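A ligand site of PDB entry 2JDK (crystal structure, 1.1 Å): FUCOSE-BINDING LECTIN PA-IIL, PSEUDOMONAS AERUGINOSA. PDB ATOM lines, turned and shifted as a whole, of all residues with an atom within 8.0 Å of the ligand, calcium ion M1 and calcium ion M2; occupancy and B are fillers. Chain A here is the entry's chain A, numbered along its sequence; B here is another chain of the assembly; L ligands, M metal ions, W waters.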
ATOM      1  N   ALA A  21      24.384 -10.331 -15.583  1.00  0.00           N
ATOM      2  CA  ALA A  21      23.778 -10.040 -14.277  1.00  0.00           C
ATOM      3  C   ALA A  21      22.597  -9.057 -14.413  1.00  0.00           C
ATOM      4  O   ALA A  21      22.649  -8.089 -15.191  1.00  0.00           O
ATOM      5  CB  ALA A  21      24.814  -9.476 -13.300  1.00  0.00           C
ATOM      6  N   ASN A  22      21.568  -9.313 -13.600  1.00  0.00           N
ATOM      7  CA  ASN A  22      20.354  -8.450 -13.550  1.00  0.00           C
ATOM      8  C   ASN A  22      19.811  -8.453 -12.142  1.00  0.00           C
ATOM      9  O   ASN A  22      18.752  -9.073 -11.861  1.00  0.00           O
ATOM     10  CB  ASN A  22      19.283  -8.962 -14.493  1.00  0.00           C
ATOM     11  CG  ASN A  22      19.634  -8.756 -15.956  1.00  0.00           C
ATOM     12  OD1 ASN A  22      19.548  -7.668 -16.512  1.00  0.00           O
ATOM     13  ND2 ASN A  22      20.082  -9.860 -16.578  1.00  0.00           N
ATOM     14  N   SER A  23      20.500  -7.775 -11.205  1.00  0.00           N
ATOM     15  CA  SER A  23      20.097  -7.851  -9.804  1.00  0.00           C
ATOM     16  C   SER A  23      20.856  -6.768  -9.036  1.00  0.00           C
ATOM     17  O   SER A  23      21.974  -6.396  -9.390  1.00  0.00           O
ATOM     18  CB  SER A  23      20.492  -9.225  -9.213  1.00  0.00           C
ATOM     19  OG  SER A  23      20.227  -9.232  -7.800  1.00  0.00           O
ATOM     20  N   SER A  24      20.285  -6.334  -7.923  1.00  0.00           N
ATOM     21  CA  SER A  24      21.038  -5.518  -6.969  1.00  0.00           C
ATOM     22  C   SER A  24      22.257  -6.221  -6.402  1.00  0.00           C
ATOM     23  O   SER A  24      23.228  -5.547  -5.997  1.00  0.00           O
ATOM     24  CB  SER A  24      20.119  -5.101  -5.815  1.00  0.00           C
ATOM     25  OG  SER A  24      19.776  -6.271  -4.978  1.00  0.00           O
ATOM     26  N   GLY A  25      22.207  -7.550  -6.317  1.00  0.00           N
ATOM     27  CA  GLY A  25      23.229  -8.273  -5.595  1.00  0.00           C
ATOM     28  C   GLY A  25      24.377  -8.734  -6.500  1.00  0.00           C
ATOM     29  O   GLY A  25      24.183  -9.016  -7.700  1.00  0.00           O
ATOM     30  N   GLN A  27      26.651 -11.249  -8.141  1.00  0.00           N
ATOM     31  CA  GLN A  27      26.535 -12.639  -8.536  1.00  0.00           C
ATOM     32  C   GLN A  27      27.928 -13.270  -8.596  1.00  0.00           C
ATOM     33  O   GLN A  27      28.849 -12.691  -9.191  1.00  0.00           O
ATOM     34  CB  GLN A  27      25.929 -12.748  -9.960  1.00  0.00           C
ATOM     35  CG  GLN A  27      24.643 -11.921 -10.117  1.00  0.00           C
ATOM     36  CD  GLN A  27      23.474 -12.447  -9.304  1.00  0.00           C
ATOM     37  OE1 GLN A  27      23.118 -13.607  -9.456  1.00  0.00           O
ATOM     38  NE2 GLN A  27      22.842 -11.589  -8.506  1.00  0.00           N
ATOM     39  N   GLN A  44      28.243  -7.230 -10.634  1.00  0.00           N
ATOM     40  CA  GLN A  44      26.947  -6.704 -10.280  1.00  0.00           C
ATOM     41  C   GLN A  44      26.468  -5.781 -11.398  1.00  0.00           C
ATOM     42  O   GLN A  44      27.199  -4.886 -11.837  1.00  0.00           O
ATOM     43  CB  GLN A  44      26.998  -5.971  -8.923  1.00  0.00           C
ATOM     44  CG  GLN A  44      25.656  -5.495  -8.367  1.00  0.00           C
ATOM     45  CD  GLN A  44      25.167  -4.201  -9.023  1.00  0.00           C
ATOM     46  OE1 GLN A  44      25.925  -3.259  -9.201  1.00  0.00           O
ATOM     47  NE2 GLN A  44      23.864  -4.131  -9.336  1.00  0.00           N
ATOM     48  N   SER A  45      25.233  -5.990 -11.834  1.00  0.00           N
ATOM     49  CA  SER A  45      24.584  -5.129 -12.812  1.00  0.00           C
ATOM     50  C   SER A  45      23.073  -5.310 -12.700  1.00  0.00           C
ATOM     51  O   SER A  45      22.637  -6.431 -12.450  1.00  0.00           O
ATOM     52  CB  SER A  45      25.025  -5.553 -14.217  1.00  0.00           C
ATOM     53  OG  SER A  45      24.413  -4.773 -15.229  1.00  0.00           O
ATOM     54  N   THR A  46      22.342  -4.243 -12.962  1.00  0.00           N
ATOM     55  CA  THR A  46      20.913  -4.329 -13.203  1.00  0.00           C
ATOM     56  C   THR A  46      20.587  -4.086 -14.670  1.00  0.00           C
ATOM     57  O   THR A  46      19.417  -3.877 -15.043  1.00  0.00           O
ATOM     58  CB  THR A  46      20.070  -3.395 -12.308  1.00  0.00           C
ATOM     59  OG1 THR A  46      20.652  -2.095 -12.386  1.00  0.00           O
ATOM     60  CG2 THR A  46      20.065  -3.883 -10.890  1.00  0.00           C
ATOM     61  N   VAL A  70      24.706 -15.739  -4.345  1.00  0.00           N
ATOM     62  CA  VAL A  70      24.518 -14.294  -4.140  1.00  0.00           C
ATOM     63  C   VAL A  70      24.322 -14.100  -2.647  1.00  0.00           C
ATOM     64  O   VAL A  70      23.542 -14.824  -2.009  1.00  0.00           O
ATOM     65  CB  VAL A  70      23.273 -13.796  -4.872  1.00  0.00           C
ATOM     66  CG1 VAL A  70      23.116 -12.252  -4.714  1.00  0.00           C
ATOM     67  CG2 VAL A  70      23.334 -14.177  -6.343  1.00  0.00           C
ATOM     68  N   SER A  95      18.598 -17.933 -12.889  1.00  0.00           N
ATOM     69  CA  SER A  95      18.767 -18.079 -11.445  1.00  0.00           C
ATOM     70  C   SER A  95      18.032 -16.971 -10.739  1.00  0.00           C
ATOM     71  O   SER A  95      17.921 -15.850 -11.247  1.00  0.00           O
ATOM     72  CB  SER A  95      20.253 -18.121 -11.061  1.00  0.00           C
ATOM     73  OG  SER A  95      20.891 -16.864 -11.351  1.00  0.00           O
ATOM     74  N   GLU A  96      17.553 -17.325  -9.545  1.00  0.00           N
ATOM     75  CA  GLU A  96      16.795 -16.398  -8.701  1.00  0.00           C
ATOM     76  C   GLU A  96      17.445 -16.264  -7.356  1.00  0.00           C
ATOM     77  O   GLU A  96      17.594 -17.248  -6.626  1.00  0.00           O
ATOM     78  CB  GLU A  96      15.327 -16.859  -8.567  1.00  0.00           C
ATOM     79  CG  GLU A  96      14.474 -15.969  -7.667  1.00  0.00           C
ATOM     80  CD  GLU A  96      14.490 -14.541  -8.121  1.00  0.00           C
ATOM     81  OE1 GLU A  96      14.262 -14.251  -9.345  1.00  0.00           O
ATOM     82  OE2 GLU A  96      14.741 -13.615  -7.298  1.00  0.00           O
ATOM     83  N   ASP A  97      17.801 -15.032  -7.002  1.00  0.00           N
ATOM     84  CA  ASP A  97      18.473 -14.728  -5.725  1.00  0.00           C
ATOM     85  C   ASP A  97      17.556 -14.144  -4.678  1.00  0.00           C
ATOM     86  O   ASP A  97      18.030 -13.873  -3.559  1.00  0.00           O
ATOM     87  CB  ASP A  97      19.681 -13.790  -5.998  1.00  0.00           C
ATOM     88  CG  ASP A  97      19.329 -12.383  -6.448  1.00  0.00           C
ATOM     89  OD1 ASP A  97      18.220 -11.897  -6.129  1.00  0.00           O
ATOM     90  OD2 ASP A  97      20.229 -11.768  -7.091  1.00  0.00           O
ATOM     91  N   GLY A  98      16.292 -13.945  -4.988  1.00  0.00           N
ATOM     92  CA  GLY A  98      15.381 -13.164  -4.136  1.00  0.00           C
ATOM     93  C   GLY A  98      13.987 -13.723  -4.204  1.00  0.00           C
ATOM     94  O   GLY A  98      13.780 -14.941  -4.197  1.00  0.00           O
ATOM     95  N   THR A  99      13.022 -12.816  -4.296  1.00  0.00           N
ATOM     96  CA  THR A  99      11.614 -13.141  -4.107  1.00  0.00           C
ATOM     97  C   THR A  99      10.763 -12.830  -5.312  1.00  0.00           C
ATOM     98  O   THR A  99       9.587 -13.247  -5.332  1.00  0.00           O
ATOM     99  CB  THR A  99      11.023 -12.464  -2.851  1.00  0.00           C
ATOM    100  OG1 THR A  99      11.118 -11.043  -3.017  1.00  0.00           O
ATOM    101  CG2 THR A  99      11.834 -12.904  -1.590  1.00  0.00           C
ATOM    102  N   ASP A 100      11.268 -12.099  -6.302  1.00  0.00           N
ATOM    103  CA  ASP A 100      10.423 -11.672  -7.392  1.00  0.00           C
ATOM    104  C   ASP A 100      10.241 -12.710  -8.503  1.00  0.00           C
ATOM    105  O   ASP A 100       9.388 -12.547  -9.394  1.00  0.00           O
ATOM    106  CB  ASP A 100      10.830 -10.331  -8.001  1.00  0.00           C
ATOM    107  CG  ASP A 100      12.180 -10.374  -8.731  1.00  0.00           C
ATOM    108  OD1 ASP A 100      12.896 -11.362  -8.544  1.00  0.00           O
ATOM    109  OD2 ASP A 100      12.492  -9.384  -9.402  1.00  0.00           O
ATOM    110  N   ASN A 101      11.062 -13.735  -8.482  1.00  0.00           N
ATOM    111  CA  ASN A 101      10.911 -14.829  -9.472  1.00  0.00           C
ATOM    112  C   ASN A 101      11.050 -14.395 -10.889  1.00  0.00           C
ATOM    113  O   ASN A 101      10.407 -14.951 -11.769  1.00  0.00           O
ATOM    114  CB  ASN A 101       9.673 -15.695  -9.185  1.00  0.00           C
ATOM    115  CG  ASN A 101       9.759 -16.333  -7.829  1.00  0.00           C
ATOM    116  OD1 ASN A 101      10.871 -16.597  -7.319  1.00  0.00           O
ATOM    117  ND2 ASN A 101       8.615 -16.600  -7.226  1.00  0.00           N
ATOM    118  N   ASP A 102      11.941 -13.429 -11.161  1.00  0.00           N
ATOM    119  CA  ASP A 102      12.272 -13.109 -12.554  1.00  0.00           C
ATOM    120  C   ASP A 102      13.322 -14.079 -13.138  1.00  0.00           C
ATOM    121  O   ASP A 102      13.419 -14.191 -14.359  1.00  0.00           O
ATOM    122  CB  ASP A 102      12.613 -11.615 -12.806  1.00  0.00           C
ATOM    123  CG  ASP A 102      13.875 -11.115 -12.060  1.00  0.00           C
ATOM    124  OD1 ASP A 102      14.474 -11.879 -11.274  1.00  0.00           O
ATOM    125  OD2 ASP A 102      14.192  -9.917 -12.326  1.00  0.00           O
ATOM    126  N   TYR A 103      14.079 -14.763 -12.275  1.00  0.00           N
ATOM    127  CA  TYR A 103      15.025 -15.788 -12.732  1.00  0.00           C
ATOM    128  C   TYR A 103      16.070 -15.273 -13.728  1.00  0.00           C
ATOM    129  O   TYR A 103      16.632 -16.065 -14.454  1.00  0.00           O
ATOM    130  CB  TYR A 103      14.313 -17.060 -13.238  1.00  0.00           C
ATOM    131  CG  TYR A 103      13.883 -17.926 -12.058  1.00  0.00           C
ATOM    132  CD1 TYR A 103      14.713 -18.897 -11.574  1.00  0.00           C
ATOM    133  CD2 TYR A 103      12.671 -17.706 -11.450  1.00  0.00           C
ATOM    134  CE1 TYR A 103      14.369 -19.632 -10.439  1.00  0.00           C
ATOM    135  CE2 TYR A 103      12.332 -18.444 -10.307  1.00  0.00           C
ATOM    136  CZ  TYR A 103      13.187 -19.396  -9.819  1.00  0.00           C
ATOM    137  OH  TYR A 103      12.811 -20.087  -8.678  1.00  0.00           O
ATOM    138  N   ASN A 104      16.372 -13.975 -13.669  1.00  0.00           N
ATOM    139  CA  ASN A 104      17.401 -13.411 -14.570  1.00  0.00           C
ATOM    140  C   ASN A 104      18.588 -12.864 -13.791  1.00  0.00           C
ATOM    141  O   ASN A 104      19.420 -12.159 -14.369  1.00  0.00           O
ATOM    142  CB  ASN A 104      16.787 -12.297 -15.434  1.00  0.00           C
ATOM    143  CG  ASN A 104      16.485 -11.049 -14.613  1.00  0.00           C
ATOM    144  OD1 ASN A 104      16.694 -11.036 -13.396  1.00  0.00           O
ATOM    145  ND2 ASN A 104      16.017  -9.995 -15.281  1.00  0.00           N
ATOM    146  N   ASP A 105      18.685 -13.181 -12.487  1.00  0.00           N
ATOM    147  CA  ASP A 105      19.616 -12.425 -11.630  1.00  0.00           C
ATOM    148  C   ASP A 105      21.045 -12.688 -12.041  1.00  0.00           C
ATOM    149  O   ASP A 105      21.878 -11.764 -12.114  1.00  0.00           O
ATOM    150  CB  ASP A 105      19.323 -12.766 -10.169  1.00  0.00           C
ATOM    151  CG  ASP A 105      17.915 -12.365  -9.787  1.00  0.00           C
ATOM    152  OD1 ASP A 105      17.368 -11.330 -10.249  1.00  0.00           O
ATOM    153  OD2 ASP A 105      17.274 -13.107  -8.973  1.00  0.00           O
ATOM    154  N   ALA A 106      21.333 -13.959 -12.348  1.00  0.00           N
ATOM    155  CA  ALA A 106      22.472 -14.331 -13.197  1.00  0.00           C
ATOM    156  C   ALA A 106      21.878 -15.210 -14.285  1.00  0.00           C
ATOM    157  O   ALA A 106      21.126 -16.177 -14.010  1.00  0.00           O
ATOM    158  CB  ALA A 106      23.581 -15.083 -12.498  1.00  0.00           C
ATOM    159  N   PRO B 113      13.162 -10.988 -19.440  1.00  0.00           N
ATOM    160  CA  PRO B 113      13.340  -9.575 -19.062  1.00  0.00           C
ATOM    161  C   PRO B 113      14.709  -9.342 -18.469  1.00  0.00           C
ATOM    162  O   PRO B 113      15.427 -10.253 -18.046  1.00  0.00           O
ATOM    163  CB  PRO B 113      12.231  -9.363 -18.003  1.00  0.00           C
ATOM    164  CG  PRO B 113      12.179 -10.712 -17.338  1.00  0.00           C
ATOM    165  CD  PRO B 113      12.348 -11.724 -18.440  1.00  0.00           C
ATOM    166  N   LEU B 114      15.026  -8.038 -18.381  1.00  0.00           N
ATOM    167  CA  LEU B 114      16.248  -7.549 -17.723  1.00  0.00           C
ATOM    168  C   LEU B 114      15.899  -6.934 -16.374  1.00  0.00           C
ATOM    169  O   LEU B 114      14.717  -6.805 -15.989  1.00  0.00           O
ATOM    170  CB  LEU B 114      16.916  -6.523 -18.624  1.00  0.00           C
ATOM    171  CG  LEU B 114      17.282  -7.000 -20.025  1.00  0.00           C
ATOM    172  CD1 LEU B 114      18.134  -5.912 -20.703  1.00  0.00           C
ATOM    173  CD2 LEU B 114      17.978  -8.372 -20.048  1.00  0.00           C
ATOM    174  N   GLY B 115      16.916  -6.517 -15.643  1.00  0.00           N
ATOM    175  CA  GLY B 115      16.712  -5.754 -14.393  1.00  0.00           C
ATOM    176  C   GLY B 115      16.553  -6.576 -13.140  1.00  0.00           C
ATOM    177  O   GLY B 115      16.303  -7.808 -13.185  1.00  0.00           O
ATOM    178  OXT GLY B 115      16.751  -5.930 -12.073  1.00  0.00           O
HETATM  179  C1  LIG L   1      17.166  -8.336  -6.690  1.00  0.00           C
HETATM  180  C2  LIG L   1      16.641  -9.292  -7.781  1.00  0.00           C
HETATM  181  C3  LIG L   1      15.472  -8.676  -8.474  1.00  0.00           C
HETATM  182  C4  LIG L   1      15.815  -7.346  -9.085  1.00  0.00           C
HETATM  183  C5  LIG L   1      16.436  -6.438  -8.004  1.00  0.00           C
HETATM  184  C6  LIG L   1      16.931  -5.109  -8.559  1.00  0.00           C
HETATM  185  O1  LIG L   1      16.148  -8.185  -5.726  1.00  0.00           O
HETATM  186  O2  LIG L   1      16.240 -10.557  -7.237  1.00  0.00           O
HETATM  187  O3  LIG L   1      15.054  -9.573  -9.538  1.00  0.00           O
HETATM  188  O4  LIG L   1      16.762  -7.601 -10.135  1.00  0.00           O
HETATM  189  O5  LIG L   1      17.509  -7.094  -7.327  1.00  0.00           O
HETATM  190 CA    CA M   1      16.474  -9.587 -11.574  1.00  0.00          CA
HETATM  191 CA    CA M   2      15.144 -11.970  -9.017  1.00  0.00          CA
HETATM  192  O   HOH W   1      13.778 -10.272  -5.450  1.00  0.00           O
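Of the 25 residues printed, 4 come within 4 Å of calcium ion M2.
Water W1 lies within hydrogen-bond range of the backbone NH (N) of Thr 99 (2.9 Å), an oxygen (O1) of the ligand (3.2 Å) and the backbone NH (N) of Asp 100 (3.2 Å).
Within 4 Å of the ligand: Asn 22, Ser 23, Ser 24, Glu 96, Asp 97, Asp 100, Asp 102, Asp 105 and Gly 115 of chain B. Along chain A the residues within 4 Å of the ligand span positions 22 to 105.
OG of Ser 23 lies close to O5 of the ligand, at 3.5 Å. O5 of the ligand lies within hydrogen-bond range of OG of Ser 24. N of Ser 24 is in hydrogen-bond range of O5 of the ligand (2.9 Å). O2 of the ligand lies close to OD1 of Asp 97 (2.6 Å).
Calcium ion M2 is bound by OD1 of Asp 102 (2.4 Å), OD1 of Asp 100 (2.4 Å), OE2 of Glu 96 (2.4 Å), OD2 of Asp 105 (2.4 Å), O3 of the ligand (2.5 Å), OE1 of Glu 96 (2.5 Å), O2 of the ligand (2.5 Å) and OD1 of Asp 105 (2.6 Å). Calcium ion M2 has eight donor atoms within binding distance.
OD2 of Asp 97 is in hydrogen-bond range of NE2 of Gln 27 (3.0 Å). ND2 of Asn 104 is in hydrogen-bond range of O of Pro 113 of chain B (2.8 Å). OE2 of Glu 96 sits close to N of Gly 98. The backbone NH (N) of Tyr 103 lies close to the side-chain carboxylate (OE1) of Glu 96 (3.0 Å). O of Ser 95 sits at hydrogen-bond distance from N of Asp 105, 3.0 Å away. The backbone carbonyl oxygen (O) of Ser 23 lies within hydrogen-bond range of the side-chain amide nitrogen (NE2) of Gln 44 (3.0 Å). The backbone NH of Asn 101 sits close to the side-chain carboxylate of Glu 96, 3.4 Å away. O of Ser 45 lies close to N of Asn 22, 3.3 Å away.
The nearest printed residue that does not touch calcium ion M1 is Ser 23 (4.4 Å).
OD1 of Asn 104 is bound to calcium ion M1. O of Asn 22 binds calcium ion M1 (2.4 Å). OD1 of Asp 105 is bound to calcium ion M1 (2.4 Å). The chain-end carboxylate (O) of Gly 115 of chain B is bound to calcium ion M1. The side-chain carboxylate (OD2) of Asp 102 is bound to calcium ion M1 (2.4 Å). An oxygen (O4) of the ligand is bound to calcium ion M1, at 2.5 Å. O3 of the ligand is bound to calcium ion M1 (2.5 Å). Slightly farther from calcium ion M1 lies OD1 of Asp 102 (3.1 Å).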
